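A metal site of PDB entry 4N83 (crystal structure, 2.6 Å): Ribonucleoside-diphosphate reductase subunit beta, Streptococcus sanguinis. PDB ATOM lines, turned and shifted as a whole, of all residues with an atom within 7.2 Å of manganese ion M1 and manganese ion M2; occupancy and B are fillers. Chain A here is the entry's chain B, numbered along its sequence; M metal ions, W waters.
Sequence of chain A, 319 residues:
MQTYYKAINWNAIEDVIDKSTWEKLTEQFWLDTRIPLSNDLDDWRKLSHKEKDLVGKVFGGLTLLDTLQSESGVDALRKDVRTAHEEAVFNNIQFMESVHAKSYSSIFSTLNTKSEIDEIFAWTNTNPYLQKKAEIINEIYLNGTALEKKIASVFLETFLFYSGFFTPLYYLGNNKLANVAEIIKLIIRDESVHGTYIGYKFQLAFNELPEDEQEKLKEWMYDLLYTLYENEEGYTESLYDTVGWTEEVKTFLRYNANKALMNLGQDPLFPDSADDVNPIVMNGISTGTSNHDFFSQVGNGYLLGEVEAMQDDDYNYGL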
ATOM      1  N   LEU A  62     -18.748 -21.785 -15.399  1.00  0.00           N
ATOM      2  CA  LEU A  62     -19.159 -22.721 -14.371  1.00  0.00           C
ATOM      3  C   LEU A  62     -19.866 -23.943 -14.969  1.00  0.00           C
ATOM      4  O   LEU A  62     -19.718 -25.056 -14.462  1.00  0.00           O
ATOM      5  CB  LEU A  62     -20.057 -22.005 -13.344  1.00  0.00           C
ATOM      6  CG  LEU A  62     -19.399 -20.854 -12.565  1.00  0.00           C
ATOM      7  CD1 LEU A  62     -20.453 -19.949 -11.933  1.00  0.00           C
ATOM      8  CD2 LEU A  62     -18.449 -21.357 -11.483  1.00  0.00           C
ATOM      9  N   LEU A  65     -17.386 -26.694 -16.148  1.00  0.00           N
ATOM     10  CA  LEU A  65     -16.635 -27.414 -15.137  1.00  0.00           C
ATOM     11  C   LEU A  65     -17.513 -28.327 -14.315  1.00  0.00           C
ATOM     12  O   LEU A  65     -17.076 -29.402 -13.907  1.00  0.00           O
ATOM     13  CB  LEU A  65     -15.914 -26.426 -14.221  1.00  0.00           C
ATOM     14  CG  LEU A  65     -14.905 -25.554 -14.990  1.00  0.00           C
ATOM     15  CD1 LEU A  65     -14.645 -24.266 -14.221  1.00  0.00           C
ATOM     16  CD2 LEU A  65     -13.627 -26.327 -15.274  1.00  0.00           C
ATOM     17  N   ASP A  66     -18.740 -27.896 -14.036  1.00  0.00           N
ATOM     18  CA  ASP A  66     -19.745 -28.785 -13.460  1.00  0.00           C
ATOM     19  C   ASP A  66     -20.115 -29.894 -14.452  1.00  0.00           C
ATOM     20  O   ASP A  66     -20.412 -31.015 -14.035  1.00  0.00           O
ATOM     21  CB  ASP A  66     -21.000 -28.019 -13.012  1.00  0.00           C
ATOM     22  CG  ASP A  66     -20.985 -27.693 -11.514  1.00  0.00           C
ATOM     23  OD1 ASP A  66     -20.459 -28.512 -10.737  1.00  0.00           O
ATOM     24  OD2 ASP A  66     -21.529 -26.632 -11.118  1.00  0.00           O
ATOM     25  N   THR A  67     -20.084 -29.585 -15.751  1.00  0.00           N
ATOM     26  CA  THR A  67     -20.202 -30.619 -16.788  1.00  0.00           C
ATOM     27  C   THR A  67     -19.066 -31.614 -16.628  1.00  0.00           C
ATOM     28  O   THR A  67     -19.295 -32.817 -16.572  1.00  0.00           O
ATOM     29  CB  THR A  67     -20.207 -30.007 -18.218  1.00  0.00           C
ATOM     30  OG1 THR A  67     -21.388 -29.242 -18.420  1.00  0.00           O
ATOM     31  CG2 THR A  67     -20.142 -31.083 -19.288  1.00  0.00           C
ATOM     32  N   GLN A  69     -17.341 -32.307 -14.000  1.00  0.00           N
ATOM     33  CA  GLN A  69     -17.513 -33.039 -12.751  1.00  0.00           C
ATOM     34  C   GLN A  69     -18.562 -34.157 -12.831  1.00  0.00           C
ATOM     35  O   GLN A  69     -18.442 -35.170 -12.147  1.00  0.00           O
ATOM     36  CB  GLN A  69     -17.900 -32.076 -11.631  1.00  0.00           C
ATOM     37  CG  GLN A  69     -16.771 -31.133 -11.210  1.00  0.00           C
ATOM     38  CD  GLN A  69     -15.599 -31.861 -10.580  1.00  0.00           C
ATOM     39  OE1 GLN A  69     -14.793 -32.482 -11.283  1.00  0.00           O
ATOM     40  NE2 GLN A  69     -15.478 -31.759  -9.267  1.00  0.00           N
ATOM     41  N   SER A  70     -19.585 -33.961 -13.663  1.00  0.00           N
ATOM     42  CA  SER A  70     -20.679 -34.904 -13.784  1.00  0.00           C
ATOM     43  C   SER A  70     -20.355 -36.048 -14.743  1.00  0.00           C
ATOM     44  O   SER A  70     -21.006 -37.098 -14.692  1.00  0.00           O
ATOM     45  CB  SER A  70     -21.920 -34.162 -14.281  1.00  0.00           C
ATOM     46  OG  SER A  70     -21.752 -33.782 -15.641  1.00  0.00           O
ATOM     47  N   VAL A  74     -16.359 -37.232 -11.013  1.00  0.00           N
ATOM     48  CA  VAL A  74     -16.803 -38.210 -10.016  1.00  0.00           C
ATOM     49  C   VAL A  74     -16.536 -39.634 -10.479  1.00  0.00           C
ATOM     50  O   VAL A  74     -16.298 -40.526  -9.664  1.00  0.00           O
ATOM     51  CB  VAL A  74     -18.309 -38.033  -9.690  1.00  0.00           C
ATOM     52  CG1 VAL A  74     -18.773 -39.124  -8.734  1.00  0.00           C
ATOM     53  CG2 VAL A  74     -18.565 -36.663  -9.087  1.00  0.00           C
ATOM     54  N   ILE A  93     -23.479 -37.554  -5.481  1.00  0.00           N
ATOM     55  CA  ILE A  93     -22.657 -36.418  -5.903  1.00  0.00           C
ATOM     56  C   ILE A  93     -22.673 -36.291  -7.429  1.00  0.00           C
ATOM     57  O   ILE A  93     -22.922 -35.218  -7.952  1.00  0.00           O
ATOM     58  CB  ILE A  93     -21.212 -36.520  -5.361  1.00  0.00           C
ATOM     59  CG1 ILE A  93     -21.194 -36.312  -3.845  1.00  0.00           C
ATOM     60  CG2 ILE A  93     -20.317 -35.484  -6.024  1.00  0.00           C
ATOM     61  CD1 ILE A  93     -19.939 -36.779  -3.145  1.00  0.00           C
ATOM     62  N   MET A  96     -25.928 -34.912  -8.626  1.00  0.00           N
ATOM     63  CA  MET A  96     -26.112 -33.504  -8.277  1.00  0.00           C
ATOM     64  C   MET A  96     -25.217 -32.569  -9.083  1.00  0.00           C
ATOM     65  O   MET A  96     -25.564 -31.409  -9.232  1.00  0.00           O
ATOM     66  CB  MET A  96     -25.914 -33.289  -6.779  1.00  0.00           C
ATOM     67  CG  MET A  96     -26.996 -33.958  -5.938  1.00  0.00           C
ATOM     68  SD  MET A  96     -28.697 -33.535  -6.374  1.00  0.00           S
ATOM     69  CE  MET A  96     -28.791 -31.803  -5.938  1.00  0.00           C
ATOM     70  N   GLU A  97     -24.110 -33.079  -9.616  1.00  0.00           N
ATOM     71  CA  GLU A  97     -23.288 -32.313 -10.540  1.00  0.00           C
ATOM     72  C   GLU A  97     -24.019 -32.060 -11.862  1.00  0.00           C
ATOM     73  O   GLU A  97     -23.836 -31.007 -12.489  1.00  0.00           O
ATOM     74  CB  GLU A  97     -21.962 -33.007 -10.825  1.00  0.00           C
ATOM     75  CG  GLU A  97     -21.029 -33.191  -9.641  1.00  0.00           C
ATOM     76  CD  GLU A  97     -20.589 -31.899  -8.986  1.00  0.00           C
ATOM     77  OE1 GLU A  97     -21.014 -30.813  -9.423  1.00  0.00           O
ATOM     78  OE2 GLU A  97     -19.813 -31.985  -8.015  1.00  0.00           O
ATOM     79  N   SER A  98     -24.831 -33.029 -12.299  1.00  0.00           N
ATOM     80  CA  SER A  98     -25.684 -32.852 -13.479  1.00  0.00           C
ATOM     81  C   SER A  98     -26.796 -31.835 -13.239  1.00  0.00           C
ATOM     82  O   SER A  98     -27.181 -31.106 -14.144  1.00  0.00           O
ATOM     83  CB  SER A  98     -26.266 -34.191 -13.952  1.00  0.00           C
ATOM     84  OG  SER A  98     -25.298 -34.929 -14.677  1.00  0.00           O
ATOM     85  N   HIS A 100     -26.368 -29.375 -11.179  1.00  0.00           N
ATOM     86  CA  HIS A 100     -25.613 -28.132 -11.150  1.00  0.00           C
ATOM     87  C   HIS A 100     -25.435 -27.596 -12.570  1.00  0.00           C
ATOM     88  O   HIS A 100     -25.806 -26.460 -12.860  1.00  0.00           O
ATOM     89  CB  HIS A 100     -24.243 -28.324 -10.483  1.00  0.00           C
ATOM     90  CG  HIS A 100     -24.321 -28.618  -9.021  1.00  0.00           C
ATOM     91  ND1 HIS A 100     -23.265 -29.137  -8.314  1.00  0.00           N
ATOM     92  CD2 HIS A 100     -25.330 -28.470  -8.138  1.00  0.00           C
ATOM     93  CE1 HIS A 100     -23.620 -29.282  -7.043  1.00  0.00           C
ATOM     94  NE2 HIS A 100     -24.869 -28.884  -6.919  1.00  0.00           N
ATOM     95  N   ALA A 101     -24.873 -28.432 -13.434  1.00  0.00           N
ATOM     96  CA  ALA A 101     -24.662 -28.083 -14.836  1.00  0.00           C
ATOM     97  C   ALA A 101     -25.951 -27.592 -15.486  1.00  0.00           C
ATOM     98  O   ALA A 101     -25.969 -26.545 -16.134  1.00  0.00           O
ATOM     99  CB  ALA A 101     -24.104 -29.275 -15.594  1.00  0.00           C
ATOM    100  N   TYR A 104     -27.684 -23.932 -14.654  1.00  0.00           N
ATOM    101  CA  TYR A 104     -27.186 -22.796 -15.432  1.00  0.00           C
ATOM    102  C   TYR A 104     -27.998 -22.602 -16.694  1.00  0.00           C
ATOM    103  O   TYR A 104     -28.240 -21.462 -17.105  1.00  0.00           O
ATOM    104  CB  TYR A 104     -25.706 -22.987 -15.782  1.00  0.00           C
ATOM    105  CG  TYR A 104     -24.818 -23.196 -14.571  1.00  0.00           C
ATOM    106  CD1 TYR A 104     -24.769 -22.246 -13.553  1.00  0.00           C
ATOM    107  CD2 TYR A 104     -24.028 -24.331 -14.440  1.00  0.00           C
ATOM    108  CE1 TYR A 104     -23.965 -22.434 -12.446  1.00  0.00           C
ATOM    109  CE2 TYR A 104     -23.216 -24.525 -13.335  1.00  0.00           C
ATOM    110  CZ  TYR A 104     -23.195 -23.575 -12.337  1.00  0.00           C
ATOM    111  OH  TYR A 104     -22.395 -23.747 -11.235  1.00  0.00           O
ATOM    112  N   SER A 153     -10.121 -32.357  -7.470  1.00  0.00           N
ATOM    113  CA  SER A 153     -11.565 -32.129  -7.373  1.00  0.00           C
ATOM    114  C   SER A 153     -11.898 -31.114  -6.262  1.00  0.00           C
ATOM    115  O   SER A 153     -12.866 -30.367  -6.378  1.00  0.00           O
ATOM    116  CB  SER A 153     -12.313 -33.441  -7.140  1.00  0.00           C
ATOM    117  OG  SER A 153     -13.713 -33.217  -7.098  1.00  0.00           O
ATOM    118  N   GLU A 157     -13.653 -27.165  -6.951  1.00  0.00           N
ATOM    119  CA  GLU A 157     -14.988 -26.737  -6.511  1.00  0.00           C
ATOM    120  C   GLU A 157     -15.045 -26.074  -5.132  1.00  0.00           C
ATOM    121  O   GLU A 157     -16.080 -25.528  -4.749  1.00  0.00           O
ATOM    122  CB  GLU A 157     -15.979 -27.891  -6.605  1.00  0.00           C
ATOM    123  CG  GLU A 157     -16.539 -28.068  -8.007  1.00  0.00           C
ATOM    124  CD  GLU A 157     -17.553 -29.182  -8.099  1.00  0.00           C
ATOM    125  OE1 GLU A 157     -17.232 -30.320  -7.713  1.00  0.00           O
ATOM    126  OE2 GLU A 157     -18.685 -28.917  -8.561  1.00  0.00           O
ATOM    127  N   PHE A 161     -13.870 -22.453  -8.418  1.00  0.00           N
ATOM    128  CA  PHE A 161     -15.241 -22.052  -8.776  1.00  0.00           C
ATOM    129  C   PHE A 161     -15.598 -20.648  -8.282  1.00  0.00           C
ATOM    130  O   PHE A 161     -16.515 -20.004  -8.826  1.00  0.00           O
ATOM    131  CB  PHE A 161     -16.281 -23.051  -8.260  1.00  0.00           C
ATOM    132  CG  PHE A 161     -16.755 -24.041  -9.295  1.00  0.00           C
ATOM    133  CD1 PHE A 161     -18.083 -24.083  -9.677  1.00  0.00           C
ATOM    134  CD2 PHE A 161     -15.869 -24.942  -9.885  1.00  0.00           C
ATOM    135  CE1 PHE A 161     -18.524 -24.996 -10.620  1.00  0.00           C
ATOM    136  CE2 PHE A 161     -16.309 -25.855 -10.827  1.00  0.00           C
ATOM    137  CZ  PHE A 161     -17.640 -25.886 -11.196  1.00  0.00           C
ATOM    138  N   PHE A 165     -18.309 -17.650  -8.582  1.00  0.00           N
ATOM    139  CA  PHE A 165     -19.372 -17.419  -7.589  1.00  0.00           C
ATOM    140  C   PHE A 165     -19.369 -16.009  -7.011  1.00  0.00           C
ATOM    141  O   PHE A 165     -20.403 -15.535  -6.534  1.00  0.00           O
ATOM    142  CB  PHE A 165     -19.297 -18.431  -6.434  1.00  0.00           C
ATOM    143  CG  PHE A 165     -19.650 -19.860  -6.821  1.00  0.00           C
ATOM    144  CD1 PHE A 165     -20.636 -20.144  -7.760  1.00  0.00           C
ATOM    145  CD2 PHE A 165     -19.021 -20.924  -6.182  1.00  0.00           C
ATOM    146  CE1 PHE A 165     -20.950 -21.455  -8.084  1.00  0.00           C
ATOM    147  CE2 PHE A 165     -19.342 -22.233  -6.494  1.00  0.00           C
ATOM    148  CZ  PHE A 165     -20.309 -22.503  -7.441  1.00  0.00           C
ATOM    149  N   ILE A 187     -26.057 -24.666  -4.940  1.00  0.00           N
ATOM    150  CA  ILE A 187     -24.882 -25.327  -5.499  1.00  0.00           C
ATOM    151  C   ILE A 187     -23.743 -25.288  -4.482  1.00  0.00           C
ATOM    152  O   ILE A 187     -23.055 -26.285  -4.285  1.00  0.00           O
ATOM    153  CB  ILE A 187     -24.423 -24.650  -6.812  1.00  0.00           C
ATOM    154  CG1 ILE A 187     -25.472 -24.879  -7.909  1.00  0.00           C
ATOM    155  CG2 ILE A 187     -23.058 -25.188  -7.243  1.00  0.00           C
ATOM    156  CD1 ILE A 187     -25.149 -24.242  -9.236  1.00  0.00           C
ATOM    157  N   ASP A 190     -24.089 -27.736  -1.639  1.00  0.00           N
ATOM    158  CA  ASP A 190     -23.671 -29.086  -2.017  1.00  0.00           C
ATOM    159  C   ASP A 190     -22.158 -29.166  -2.055  1.00  0.00           C
ATOM    160  O   ASP A 190     -21.575 -30.110  -1.525  1.00  0.00           O
ATOM    161  CB  ASP A 190     -24.250 -29.479  -3.386  1.00  0.00           C
ATOM    162  CG  ASP A 190     -25.761 -29.618  -3.368  1.00  0.00           C
ATOM    163  OD1 ASP A 190     -26.321 -29.813  -2.277  1.00  0.00           O
ATOM    164  OD2 ASP A 190     -26.370 -29.528  -4.463  1.00  0.00           O
ATOM    165  N   GLU A 191     -21.527 -28.181  -2.687  1.00  0.00           N
ATOM    166  CA  GLU A 191     -20.077 -28.200  -2.902  1.00  0.00           C
ATOM    167  C   GLU A 191     -19.249 -28.093  -1.607  1.00  0.00           C
ATOM    168  O   GLU A 191     -18.111 -28.552  -1.576  1.00  0.00           O
ATOM    169  CB  GLU A 191     -19.654 -27.121  -3.900  1.00  0.00           C
ATOM    170  CG  GLU A 191     -20.139 -27.344  -5.320  1.00  0.00           C
ATOM    171  CD  GLU A 191     -19.841 -28.740  -5.829  1.00  0.00           C
ATOM    172  OE1 GLU A 191     -18.775 -29.306  -5.469  1.00  0.00           O
ATOM    173  OE2 GLU A 191     -20.662 -29.293  -6.584  1.00  0.00           O
ATOM    174  N   SER A 192     -19.792 -27.488  -0.560  1.00  0.00           N
ATOM    175  CA  SER A 192     -19.082 -27.404   0.703  1.00  0.00           C
ATOM    176  C   SER A 192     -18.984 -28.789   1.355  1.00  0.00           C
ATOM    177  O   SER A 192     -17.930 -29.166   1.884  1.00  0.00           O
ATOM    178  CB  SER A 192     -19.726 -26.386   1.656  1.00  0.00           C
ATOM    179  OG  SER A 192     -21.040 -26.775   1.997  1.00  0.00           O
ATOM    180  N   HIS A 194     -19.351 -31.608  -0.416  1.00  0.00           N
ATOM    181  CA  HIS A 194     -18.532 -32.360  -1.376  1.00  0.00           C
ATOM    182  C   HIS A 194     -17.046 -32.281  -1.034  1.00  0.00           C
ATOM    183  O   HIS A 194     -16.352 -33.303  -1.001  1.00  0.00           O
ATOM    184  CB  HIS A 194     -18.768 -31.849  -2.810  1.00  0.00           C
ATOM    185  CG  HIS A 194     -20.124 -32.162  -3.361  1.00  0.00           C
ATOM    186  ND1 HIS A 194     -20.463 -31.918  -4.677  1.00  0.00           N
ATOM    187  CD2 HIS A 194     -21.222 -32.717  -2.788  1.00  0.00           C
ATOM    188  CE1 HIS A 194     -21.722 -32.285  -4.875  1.00  0.00           C
ATOM    189  NE2 HIS A 194     -22.205 -32.776  -3.747  1.00  0.00           N
ATOM    190  N   GLY A 195     -16.558 -31.074  -0.771  1.00  0.00           N
ATOM    191  CA  GLY A 195     -15.145 -30.853  -0.499  1.00  0.00           C
ATOM    192  C   GLY A 195     -14.710 -31.382   0.856  1.00  0.00           C
ATOM    193  O   GLY A 195     -13.617 -31.934   0.989  1.00  0.00           O
ATOM    194  N   ILE A 198     -14.701 -35.302   0.322  1.00  0.00           N
ATOM    195  CA  ILE A 198     -13.566 -35.737  -0.493  1.00  0.00           C
ATOM    196  C   ILE A 198     -12.252 -35.463   0.237  1.00  0.00           C
ATOM    197  O   ILE A 198     -11.311 -36.252   0.145  1.00  0.00           O
ATOM    198  CB  ILE A 198     -13.544 -35.044  -1.870  1.00  0.00           C
ATOM    199  CG1 ILE A 198     -14.780 -35.412  -2.683  1.00  0.00           C
ATOM    200  CG2 ILE A 198     -12.300 -35.450  -2.652  1.00  0.00           C
ATOM    201  CD1 ILE A 198     -15.033 -34.483  -3.862  1.00  0.00           C
HETATM  202 MN    MN M   1     -18.975 -31.213  -6.542  1.00  0.00          MN
HETATM  203 MN    MN M   2     -20.960 -28.892  -8.806  1.00  0.00          MN
HETATM  204  O   HOH W   1     -20.456 -26.468  -8.520  1.00  0.00           O
HETATM  205  O   HOH W   2     -17.135 -32.665  -6.366  1.00  0.00           O
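OH of Tyr 104 lies within hydrogen-bond range of OD2 of Asp 66 (3.0 Å).
O of Asp 66 is in hydrogen-bond range of OG of Ser 70 (3.5 Å).
The backbone carbonyl oxygen (O) of Met 96 lies close to a ring nitrogen (NE2) of His 100 (3.5 Å).
OE1 of Glu 157 sits close to NE2 of Gln 69 (2.7 Å).
OD2 of Asp 190 sits at hydrogen-bond distance from NE2 of His 100, at 2.9 Å.
The nearest printed residue that does not touch manganese ion M1 is Gln 69 (4.5 Å).
Of the 25 residues printed, 5 come within 4 Å of manganese ion M2.
The nearest printed residue that does not touch manganese ion M2 is Ile 187 (4.5 Å).
Manganese ion M1 is bound by OE2 of Glu 97 (1.9 Å), OE1 of Glu 191 (2.2 Å), OE1 of Glu 157 (2.3 Å), water W2 (2.4 Å), ND1 of His 194 (2.5 Å) and OE2 of Glu 191 (2.6 Å).
Manganese ion M1 has six donor atoms within binding distance.
Manganese ion M2 is bound by the side-chain carboxylate of Glu 97, the side-chain carboxylate of Asp 66, the side-chain carboxylate of Glu 191, the side-chain carboxylate of Glu 157, a ring nitrogen (ND1) of His 100 and water W1.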
